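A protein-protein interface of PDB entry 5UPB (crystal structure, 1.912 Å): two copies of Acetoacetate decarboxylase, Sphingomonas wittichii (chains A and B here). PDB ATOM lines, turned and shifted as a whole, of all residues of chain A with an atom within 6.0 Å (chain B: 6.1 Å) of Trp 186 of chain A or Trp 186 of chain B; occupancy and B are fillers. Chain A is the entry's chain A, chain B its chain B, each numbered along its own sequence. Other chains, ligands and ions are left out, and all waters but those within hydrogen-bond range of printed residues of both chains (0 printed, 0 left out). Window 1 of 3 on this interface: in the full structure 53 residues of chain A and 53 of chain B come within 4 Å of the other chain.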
ATOM      1  N   ILE A 112     -23.237  -4.364  -2.396  1.00  0.00           N
ATOM      2  CA  ILE A 112     -22.882  -5.661  -1.859  1.00  0.00           C
ATOM      3  C   ILE A 112     -22.283  -6.565  -2.934  1.00  0.00           C
ATOM      4  O   ILE A 112     -21.277  -7.246  -2.693  1.00  0.00           O
ATOM      5  CB  ILE A 112     -24.117  -6.286  -1.192  1.00  0.00           C
ATOM      6  CG1 ILE A 112     -24.435  -5.523   0.142  1.00  0.00           C
ATOM      7  CG2 ILE A 112     -23.900  -7.778  -0.976  1.00  0.00           C
ATOM      8  CD1 ILE A 112     -23.400  -5.739   1.227  1.00  0.00           C
ATOM      9  N   TRP A 115     -18.789  -5.467  -3.105  1.00  0.00           N
ATOM     10  CA  TRP A 115     -17.923  -5.889  -2.007  1.00  0.00           C
ATOM     11  C   TRP A 115     -17.556  -7.360  -2.151  1.00  0.00           C
ATOM     12  O   TRP A 115     -16.419  -7.757  -1.863  1.00  0.00           O
ATOM     13  CB  TRP A 115     -18.593  -5.645  -0.640  1.00  0.00           C
ATOM     14  CG  TRP A 115     -18.500  -4.262  -0.046  1.00  0.00           C
ATOM     15  CD1 TRP A 115     -18.824  -3.076  -0.647  1.00  0.00           C
ATOM     16  CD2 TRP A 115     -18.088  -3.925   1.296  1.00  0.00           C
ATOM     17  NE1 TRP A 115     -18.622  -2.021   0.230  1.00  0.00           N
ATOM     18  CE2 TRP A 115     -18.182  -2.514   1.426  1.00  0.00           C
ATOM     19  CE3 TRP A 115     -17.648  -4.675   2.392  1.00  0.00           C
ATOM     20  CZ2 TRP A 115     -17.841  -1.837   2.603  1.00  0.00           C
ATOM     21  CZ3 TRP A 115     -17.313  -4.002   3.560  1.00  0.00           C
ATOM     22  CH2 TRP A 115     -17.411  -2.591   3.650  1.00  0.00           C
ATOM     23  N   LEU A 116     -18.526  -8.191  -2.563  1.00  0.00           N
ATOM     24  CA  LEU A 116     -18.268  -9.621  -2.687  1.00  0.00           C
ATOM     25  C   LEU A 116     -17.198  -9.910  -3.717  1.00  0.00           C
ATOM     26  O   LEU A 116     -16.506 -10.932  -3.634  1.00  0.00           O
ATOM     27  CB  LEU A 116     -19.539 -10.364  -3.061  1.00  0.00           C
ATOM     28  CG  LEU A 116     -20.593 -10.340  -1.943  1.00  0.00           C
ATOM     29  CD1 LEU A 116     -21.981 -10.783  -2.489  1.00  0.00           C
ATOM     30  CD2 LEU A 116     -20.165 -11.269  -0.810  1.00  0.00           C
ATOM     31  N   ASN A 117     -17.087  -9.049  -4.706  1.00  0.00           N
ATOM     32  CA  ASN A 117     -16.086  -9.154  -5.750  1.00  0.00           C
ATOM     33  C   ASN A 117     -14.922  -8.196  -5.518  1.00  0.00           C
ATOM     34  O   ASN A 117     -14.140  -7.932  -6.448  1.00  0.00           O
ATOM     35  CB  ASN A 117     -16.788  -8.887  -7.084  1.00  0.00           C
ATOM     36  CG  ASN A 117     -17.562 -10.099  -7.604  1.00  0.00           C
ATOM     37  OD1 ASN A 117     -17.193 -11.239  -7.345  1.00  0.00           O
ATOM     38  ND2 ASN A 117     -18.714  -9.847  -8.234  1.00  0.00           N
ATOM     39  N   ARG A 184     -11.208  -8.411  -1.893  1.00  0.00           N
ATOM     40  CA  ARG A 184     -12.355  -9.012  -1.236  1.00  0.00           C
ATOM     41  C   ARG A 184     -12.006  -9.103   0.231  1.00  0.00           C
ATOM     42  O   ARG A 184     -11.118  -9.870   0.618  1.00  0.00           O
ATOM     43  CB  ARG A 184     -12.717 -10.342  -1.879  1.00  0.00           C
ATOM     44  CG  ARG A 184     -13.871 -11.027  -1.224  1.00  0.00           C
ATOM     45  CD  ARG A 184     -14.164 -12.308  -1.960  1.00  0.00           C
ATOM     46  NE  ARG A 184     -15.472 -12.812  -1.581  1.00  0.00           N
ATOM     47  CZ  ARG A 184     -15.594 -13.752  -0.684  1.00  0.00           C
ATOM     48  NH1 ARG A 184     -14.508 -14.230  -0.116  1.00  0.00           N
ATOM     49  NH2 ARG A 184     -16.790 -14.217  -0.306  1.00  0.00           N
ATOM     50  N   HIS A 185     -12.673  -8.281   1.038  1.00  0.00           N
ATOM     51  CA  HIS A 185     -12.248  -8.038   2.405  1.00  0.00           C
ATOM     52  C   HIS A 185     -13.463  -8.087   3.313  1.00  0.00           C
ATOM     53  O   HIS A 185     -14.474  -7.445   3.013  1.00  0.00           O
ATOM     54  CB  HIS A 185     -11.556  -6.660   2.499  1.00  0.00           C
ATOM     55  CG  HIS A 185     -10.944  -6.388   3.839  1.00  0.00           C
ATOM     56  ND1 HIS A 185     -11.492  -5.497   4.728  1.00  0.00           N
ATOM     57  CD2 HIS A 185      -9.829  -6.881   4.434  1.00  0.00           C
ATOM     58  CE1 HIS A 185     -10.751  -5.461   5.824  1.00  0.00           C
ATOM     59  NE2 HIS A 185      -9.739  -6.297   5.675  1.00  0.00           N
ATOM     60  N   TRP A 186     -13.380  -8.875   4.388  1.00  0.00           N
ATOM     61  CA  TRP A 186     -14.504  -9.046   5.306  1.00  0.00           C
ATOM     62  C   TRP A 186     -13.917  -9.205   6.697  1.00  0.00           C
ATOM     63  O   TRP A 186     -13.632 -10.322   7.152  1.00  0.00           O
ATOM     64  CB  TRP A 186     -15.377 -10.237   4.917  1.00  0.00           C
ATOM     65  CG  TRP A 186     -16.734 -10.251   5.570  1.00  0.00           C
ATOM     66  CD1 TRP A 186     -17.240 -11.225   6.401  1.00  0.00           C
ATOM     67  CD2 TRP A 186     -17.756  -9.247   5.466  1.00  0.00           C
ATOM     68  NE1 TRP A 186     -18.519 -10.899   6.797  1.00  0.00           N
ATOM     69  CE2 TRP A 186     -18.858  -9.687   6.251  1.00  0.00           C
ATOM     70  CE3 TRP A 186     -17.856  -8.031   4.784  1.00  0.00           C
ATOM     71  CZ2 TRP A 186     -20.043  -8.949   6.371  1.00  0.00           C
ATOM     72  CZ3 TRP A 186     -19.035  -7.284   4.913  1.00  0.00           C
ATOM     73  CH2 TRP A 186     -20.118  -7.758   5.707  1.00  0.00           C
ATOM     74  N   PRO A 187     -13.668  -8.105   7.387  1.00  0.00           N
ATOM     75  CA  PRO A 187     -12.882  -8.182   8.621  1.00  0.00           C
ATOM     76  C   PRO A 187     -13.698  -8.751   9.768  1.00  0.00           C
ATOM     77  O   PRO A 187     -14.925  -8.839   9.716  1.00  0.00           O
ATOM     78  CB  PRO A 187     -12.499  -6.720   8.893  1.00  0.00           C
ATOM     79  CG  PRO A 187     -13.627  -5.937   8.272  1.00  0.00           C
ATOM     80  CD  PRO A 187     -14.008  -6.712   7.028  1.00  0.00           C
ATOM     81  N   ALA A 188     -12.974  -9.163  10.800  1.00  0.00           N
ATOM     82  CA  ALA A 188     -13.568  -9.666  12.040  1.00  0.00           C
ATOM     83  C   ALA A 188     -13.743  -8.524  13.038  1.00  0.00           C
ATOM     84  O   ALA A 188     -12.833  -7.721  13.231  1.00  0.00           O
ATOM     85  CB  ALA A 188     -12.707 -10.759  12.686  1.00  0.00           C
ATOM     86  N   THR A 194     -14.509 -15.275  11.713  1.00  0.00           N
ATOM     87  CA  THR A 194     -13.641 -15.690  10.603  1.00  0.00           C
ATOM     88  C   THR A 194     -13.446 -14.533   9.639  1.00  0.00           C
ATOM     89  O   THR A 194     -14.410 -14.131   8.984  1.00  0.00           O
ATOM     90  CB  THR A 194     -14.225 -16.872   9.852  1.00  0.00           C
ATOM     91  OG1 THR A 194     -14.473 -17.946  10.760  1.00  0.00           O
ATOM     92  CG2 THR A 194     -13.252 -17.323   8.700  1.00  0.00           C
ATOM     93  N   PRO A 195     -12.240 -13.991   9.486  1.00  0.00           N
ATOM     94  CA  PRO A 195     -12.038 -12.886   8.545  1.00  0.00           C
ATOM     95  C   PRO A 195     -11.698 -13.385   7.142  1.00  0.00           C
ATOM     96  O   PRO A 195     -11.322 -14.531   6.929  1.00  0.00           O
ATOM     97  CB  PRO A 195     -10.844 -12.146   9.156  1.00  0.00           C
ATOM     98  CG  PRO A 195     -10.013 -13.261   9.751  1.00  0.00           C
ATOM     99  CD  PRO A 195     -10.999 -14.323  10.212  1.00  0.00           C
ATOM    100  N   VAL A 196     -11.860 -12.497   6.176  1.00  0.00           N
ATOM    101  CA  VAL A 196     -11.451 -12.736   4.795  1.00  0.00           C
ATOM    102  C   VAL A 196     -10.652 -11.540   4.326  1.00  0.00           C
ATOM    103  O   VAL A 196     -11.053 -10.395   4.572  1.00  0.00           O
ATOM    104  CB  VAL A 196     -12.653 -12.943   3.840  1.00  0.00           C
ATOM    105  CG1 VAL A 196     -12.161 -13.110   2.342  1.00  0.00           C
ATOM    106  CG2 VAL A 196     -13.527 -14.106   4.281  1.00  0.00           C
ATOM    107  N   SER A 197      -9.544 -11.806   3.626  1.00  0.00           N
ATOM    108  CA  SER A 197      -8.773 -10.755   2.961  1.00  0.00           C
ATOM    109  C   SER A 197      -8.023 -11.364   1.776  1.00  0.00           C
ATOM    110  O   SER A 197      -7.019 -12.061   1.946  1.00  0.00           O
ATOM    111  CB  SER A 197      -7.810 -10.076   3.929  1.00  0.00           C
ATOM    112  OG  SER A 197      -7.116  -9.041   3.242  1.00  0.00           O
ATOM    113  N   ILE B 112     -23.369  -2.087   7.181  1.00  0.00           N
ATOM    114  CA  ILE B 112     -22.169  -2.905   7.158  1.00  0.00           C
ATOM    115  C   ILE B 112     -21.805  -3.361   8.547  1.00  0.00           C
ATOM    116  O   ILE B 112     -21.481  -4.538   8.761  1.00  0.00           O
ATOM    117  CB  ILE B 112     -21.006  -2.158   6.462  1.00  0.00           C
ATOM    118  CG1 ILE B 112     -21.283  -2.089   4.966  1.00  0.00           C
ATOM    119  CG2 ILE B 112     -19.655  -2.838   6.741  1.00  0.00           C
ATOM    120  CD1 ILE B 112     -21.216  -3.434   4.212  1.00  0.00           C
ATOM    121  N   TRP B 115     -23.995  -6.311   9.075  1.00  0.00           N
ATOM    122  CA  TRP B 115     -23.637  -7.538   8.384  1.00  0.00           C
ATOM    123  C   TRP B 115     -22.439  -8.201   9.042  1.00  0.00           C
ATOM    124  O   TRP B 115     -22.380  -9.426   9.135  1.00  0.00           O
ATOM    125  CB  TRP B 115     -23.293  -7.268   6.903  1.00  0.00           C
ATOM    126  CG  TRP B 115     -24.421  -7.179   5.988  1.00  0.00           C
ATOM    127  CD1 TRP B 115     -25.519  -6.383   6.115  1.00  0.00           C
ATOM    128  CD2 TRP B 115     -24.571  -7.877   4.738  1.00  0.00           C
ATOM    129  NE1 TRP B 115     -26.351  -6.544   5.028  1.00  0.00           N
ATOM    130  CE2 TRP B 115     -25.799  -7.464   4.176  1.00  0.00           C
ATOM    131  CE3 TRP B 115     -23.797  -8.819   4.060  1.00  0.00           C
ATOM    132  CZ2 TRP B 115     -26.271  -7.957   2.953  1.00  0.00           C
ATOM    133  CZ3 TRP B 115     -24.267  -9.315   2.845  1.00  0.00           C
ATOM    134  CH2 TRP B 115     -25.499  -8.890   2.317  1.00  0.00           C
ATOM    135  N   LEU B 116     -21.460  -7.407   9.478  1.00  0.00           N
ATOM    136  CA  LEU B 116     -20.247  -7.978  10.062  1.00  0.00           C
ATOM    137  C   LEU B 116     -20.557  -8.774  11.315  1.00  0.00           C
ATOM    138  O   LEU B 116     -19.809  -9.700  11.651  1.00  0.00           O
ATOM    139  CB  LEU B 116     -19.230  -6.880  10.393  1.00  0.00           C
ATOM    140  CG  LEU B 116     -18.651  -6.136   9.191  1.00  0.00           C
ATOM    141  CD1 LEU B 116     -17.940  -4.870   9.696  1.00  0.00           C
ATOM    142  CD2 LEU B 116     -17.726  -7.053   8.424  1.00  0.00           C
ATOM    143  N   ASN B 117     -21.615  -8.399  12.030  1.00  0.00           N
ATOM    144  CA  ASN B 117     -22.074  -9.105  13.223  1.00  0.00           C
ATOM    145  C   ASN B 117     -23.287  -9.982  12.937  1.00  0.00           C
ATOM    146  O   ASN B 117     -23.983 -10.410  13.869  1.00  0.00           O
ATOM    147  CB  ASN B 117     -22.374  -8.091  14.325  1.00  0.00           C
ATOM    148  CG  ASN B 117     -21.122  -7.614  15.039  1.00  0.00           C
ATOM    149  OD1 ASN B 117     -20.122  -8.343  15.143  1.00  0.00           O
ATOM    150  ND2 ASN B 117     -21.136  -6.355  15.460  1.00  0.00           N
ATOM    151  N   ARG B 184     -23.471 -14.395  10.492  1.00  0.00           N
ATOM    152  CA  ARG B 184     -22.399 -13.701   9.815  1.00  0.00           C
ATOM    153  C   ARG B 184     -22.101 -14.489   8.541  1.00  0.00           C
ATOM    154  O   ARG B 184     -21.559 -15.602   8.581  1.00  0.00           O
ATOM    155  CB  ARG B 184     -21.198 -13.576  10.749  1.00  0.00           C
ATOM    156  CG  ARG B 184     -20.013 -12.874  10.087  1.00  0.00           C
ATOM    157  CD  ARG B 184     -18.831 -12.716  11.028  1.00  0.00           C
ATOM    158  NE  ARG B 184     -17.835 -11.739  10.553  1.00  0.00           N
ATOM    159  CZ  ARG B 184     -16.729 -12.091   9.937  1.00  0.00           C
ATOM    160  NH1 ARG B 184     -16.479 -13.360   9.714  1.00  0.00           N
ATOM    161  NH2 ARG B 184     -15.847 -11.188   9.554  1.00  0.00           N
ATOM    162  N   HIS B 185     -22.468 -13.907   7.414  1.00  0.00           N
ATOM    163  CA  HIS B 185     -22.515 -14.619   6.145  1.00  0.00           C
ATOM    164  C   HIS B 185     -21.892 -13.752   5.064  1.00  0.00           C
ATOM    165  O   HIS B 185     -22.297 -12.600   4.871  1.00  0.00           O
ATOM    166  CB  HIS B 185     -23.968 -14.979   5.809  1.00  0.00           C
ATOM    167  CG  HIS B 185     -24.126 -15.831   4.584  1.00  0.00           C
ATOM    168  ND1 HIS B 185     -24.639 -15.341   3.402  1.00  0.00           N
ATOM    169  CD2 HIS B 185     -23.814 -17.130   4.354  1.00  0.00           C
ATOM    170  CE1 HIS B 185     -24.672 -16.315   2.510  1.00  0.00           C
ATOM    171  NE2 HIS B 185     -24.165 -17.408   3.056  1.00  0.00           N
ATOM    172  N   TRP B 186     -20.948 -14.337   4.327  1.00  0.00           N
ATOM    173  CA  TRP B 186     -20.204 -13.637   3.284  1.00  0.00           C
ATOM    174  C   TRP B 186     -19.963 -14.662   2.190  1.00  0.00           C
ATOM    175  O   TRP B 186     -18.975 -15.407   2.225  1.00  0.00           O
ATOM    176  CB  TRP B 186     -18.893 -13.063   3.828  1.00  0.00           C
ATOM    177  CG  TRP B 186     -18.292 -12.037   2.936  1.00  0.00           C
ATOM    178  CD1 TRP B 186     -17.063 -12.072   2.333  1.00  0.00           C
ATOM    179  CD2 TRP B 186     -18.914 -10.814   2.518  1.00  0.00           C
ATOM    180  NE1 TRP B 186     -16.876 -10.936   1.580  1.00  0.00           N
ATOM    181  CE2 TRP B 186     -17.993 -10.139   1.683  1.00  0.00           C
ATOM    182  CE3 TRP B 186     -20.155 -10.214   2.788  1.00  0.00           C
ATOM    183  CZ2 TRP B 186     -18.290  -8.900   1.076  1.00  0.00           C
ATOM    184  CZ3 TRP B 186     -20.443  -8.978   2.214  1.00  0.00           C
ATOM    185  CH2 TRP B 186     -19.514  -8.338   1.345  1.00  0.00           C
ATOM    186  N   PRO B 187     -20.915 -14.815   1.273  1.00  0.00           N
ATOM    187  CA  PRO B 187     -20.864 -15.948   0.346  1.00  0.00           C
ATOM    188  C   PRO B 187     -19.850 -15.743  -0.765  1.00  0.00           C
ATOM    189  O   PRO B 187     -19.499 -14.623  -1.139  1.00  0.00           O
ATOM    190  CB  PRO B 187     -22.290 -16.018  -0.219  1.00  0.00           C
ATOM    191  CG  PRO B 187     -22.772 -14.579  -0.151  1.00  0.00           C
ATOM    192  CD  PRO B 187     -22.160 -14.025   1.139  1.00  0.00           C
ATOM    193  N   ALA B 188     -19.507 -16.852  -1.396  1.00  0.00           N
ATOM    194  CA  ALA B 188     -18.600 -16.823  -2.520  1.00  0.00           C
ATOM    195  C   ALA B 188     -19.424 -16.692  -3.789  1.00  0.00           C
ATOM    196  O   ALA B 188     -20.361 -17.461  -4.007  1.00  0.00           O
ATOM    197  CB  ALA B 188     -17.753 -18.091  -2.562  1.00  0.00           C
ATOM    198  N   THR B 194     -13.229 -17.032  -0.800  1.00  0.00           N
ATOM    199  CA  THR B 194     -13.310 -17.544   0.567  1.00  0.00           C
ATOM    200  C   THR B 194     -14.634 -17.125   1.190  1.00  0.00           C
ATOM    201  O   THR B 194     -14.878 -15.920   1.336  1.00  0.00           O
ATOM    202  CB  THR B 194     -12.147 -17.023   1.406  1.00  0.00           C
ATOM    203  OG1 THR B 194     -10.895 -17.353   0.768  1.00  0.00           O
ATOM    204  CG2 THR B 194     -12.196 -17.602   2.801  1.00  0.00           C
ATOM    205  N   PRO B 195     -15.536 -18.055   1.491  1.00  0.00           N
ATOM    206  CA  PRO B 195     -16.820 -17.708   2.103  1.00  0.00           C
ATOM    207  C   PRO B 195     -16.750 -17.718   3.630  1.00  0.00           C
ATOM    208  O   PRO B 195     -15.827 -18.240   4.242  1.00  0.00           O
ATOM    209  CB  PRO B 195     -17.755 -18.808   1.586  1.00  0.00           C
ATOM    210  CG  PRO B 195     -16.866 -20.018   1.533  1.00  0.00           C
ATOM    211  CD  PRO B 195     -15.467 -19.496   1.191  1.00  0.00           C
ATOM    212  N   VAL B 196     -17.737 -17.091   4.232  1.00  0.00           N
ATOM    213  CA  VAL B 196     -17.941 -17.123   5.672  1.00  0.00           C
ATOM    214  C   VAL B 196     -19.395 -17.477   5.920  1.00  0.00           C
ATOM    215  O   VAL B 196     -20.297 -16.907   5.292  1.00  0.00           O
ATOM    216  CB  VAL B 196     -17.607 -15.765   6.320  1.00  0.00           C
ATOM    217  CG1 VAL B 196     -17.921 -15.766   7.822  1.00  0.00           C
ATOM    218  CG2 VAL B 196     -16.138 -15.416   6.078  1.00  0.00           C
ATOM    219  N   SER B 197     -19.626 -18.380   6.866  1.00  0.00           N
ATOM    220  CA  SER B 197     -20.993 -18.660   7.282  1.00  0.00           C
ATOM    221  C   SER B 197     -20.931 -19.178   8.703  1.00  0.00           C
ATOM    222  O   SER B 197     -20.531 -20.324   8.936  1.00  0.00           O
ATOM    223  CB  SER B 197     -21.657 -19.675   6.364  1.00  0.00           C
ATOM    224  OG  SER B 197     -23.009 -19.899   6.770  1.00  0.00           O
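Trp 115 of chain A touches Trp 186 of chain B, and with the chains exchanged Trp 186 of chain A touches Trp 115 of chain B. Arg 184 of chain A touches Ala 188 of chain B, and with the chains exchanged Ala 188 of chain A touches Arg 184 of chain B. Trp 186 of chain A touches its own counterpart, Trp 186 of chain B. Thr 194 of chain A touches Val 196 of chain B, and with the chains exchanged Val 196 of chain A touches Thr 194 of chain B. 13 positions are printed for both chains.
The guanidinium group of Arg 184 of chain A lies within hydrogen-bond range of the backbone carbonyl oxygen of Pro 187 of chain B, 2.9 Å away. The guanidinium group (NH2) of Arg 184 of chain A sits at hydrogen-bond distance from the backbone carbonyl oxygen (O) of Thr 194 of chain B (3.0 Å). O of Trp 186 of chain A lies within hydrogen-bond range of NH2 of Arg 184 of chain B, at 3.4 Å. The backbone carbonyl oxygen of Pro 187 of chain A lies within hydrogen-bond range of the guanidinium group of Arg 184 of chain B (2.5 Å). The backbone carbonyl oxygen (O) of Thr 194 of chain A sits close to the guanidinium group (NH2) of Arg 184 of chain B, at 3.3 Å.
Printed residues of chain B within 4 Å of Ile 112 of chain A: Trp 115. Trp 186 of chain A touches just these residues of chain B: Trp 115 (3.4 Å), Leu 116 (3.6 Å), Arg 184 (3.4 Å) and Trp 186 (3.5 Å). Of the printed residues of chain B, Thr 194 of chain A touches Arg 184 (2.3 Å) and Val 196 (3.6 Å). Trp 186 of chain B touches just these residues of chain A: Trp 115, Leu 116, Arg 184 and Trp 186. Of the printed residues of chain A, Pro 187 of chain B touches Leu 116 and Arg 184. Printed residues of chain A within 4 Å of Ala 188 of chain B: Arg 184 (3.9 Å). Of the printed residues of chain A, Thr 194 of chain B touches Arg 184 (2.3 Å) and Val 196 (3.7 Å). The nearest residue of chain B that does not touch Trp 186 of chain A is Val 196 of chain B (4.3 Å). The nearest printed residue of chain A that does not touch Trp 186 of chain B is His 185 of chain A (4.5 Å). The nearest printed residue of chain B that does not touch Ile 112 of chain A is Ile 112 of chain B (4.4 Å).
Of the 13 printed residues of chain A, 9 touch a printed residue of chain B. Hydrophobic or aromatic side chains of chain A within 4 Å of the printed part of chain B: Ile 112, Trp 115, Leu 116, Trp 186, Pro 187 and Val 196.
Among the printed residues, pairs that only touch across the chains: Ile 112 of chain A with Trp 115 of chain B, Trp 115 of chain A with Ile 112 of chain B, Trp 115 of chain A with Trp 186 of chain B, Leu 116 of chain A with Trp 186 of chain B, Leu 116 of chain A with Pro 187 of chain B, Arg 184 of chain A with Trp 186 of chain B, Arg 184 of chain A with Ala 188 of chain B, Trp 186 of chain A with Trp 115 of chain B, Trp 186 of chain A with Leu 116 of chain B, Trp 186 of chain A with Trp 186 of chain B, Pro 187 of chain A with Leu 116 of chain B, Ala 188 of chain A with Arg 184 of chain B, Thr 194 of chain A with Val 196 of chain B, Val 196 of chain A with Thr 194 of chain B and Val 196 of chain A with Val 196 of chain B.
O of Leu 116 of chain A lies within hydrogen-bond range of NE of Arg 184 of chain A. N of Trp 186 of chain A sits at hydrogen-bond distance from O of Val 196 of chain A (2.8 Å). O of Leu 116 of chain B sits at hydrogen-bond distance from NE of Arg 184 of chain B. The backbone NH of Trp 186 of chain B is in hydrogen-bond range of the backbone carbonyl oxygen of Val 196 of chain B, 2.8 Å away.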
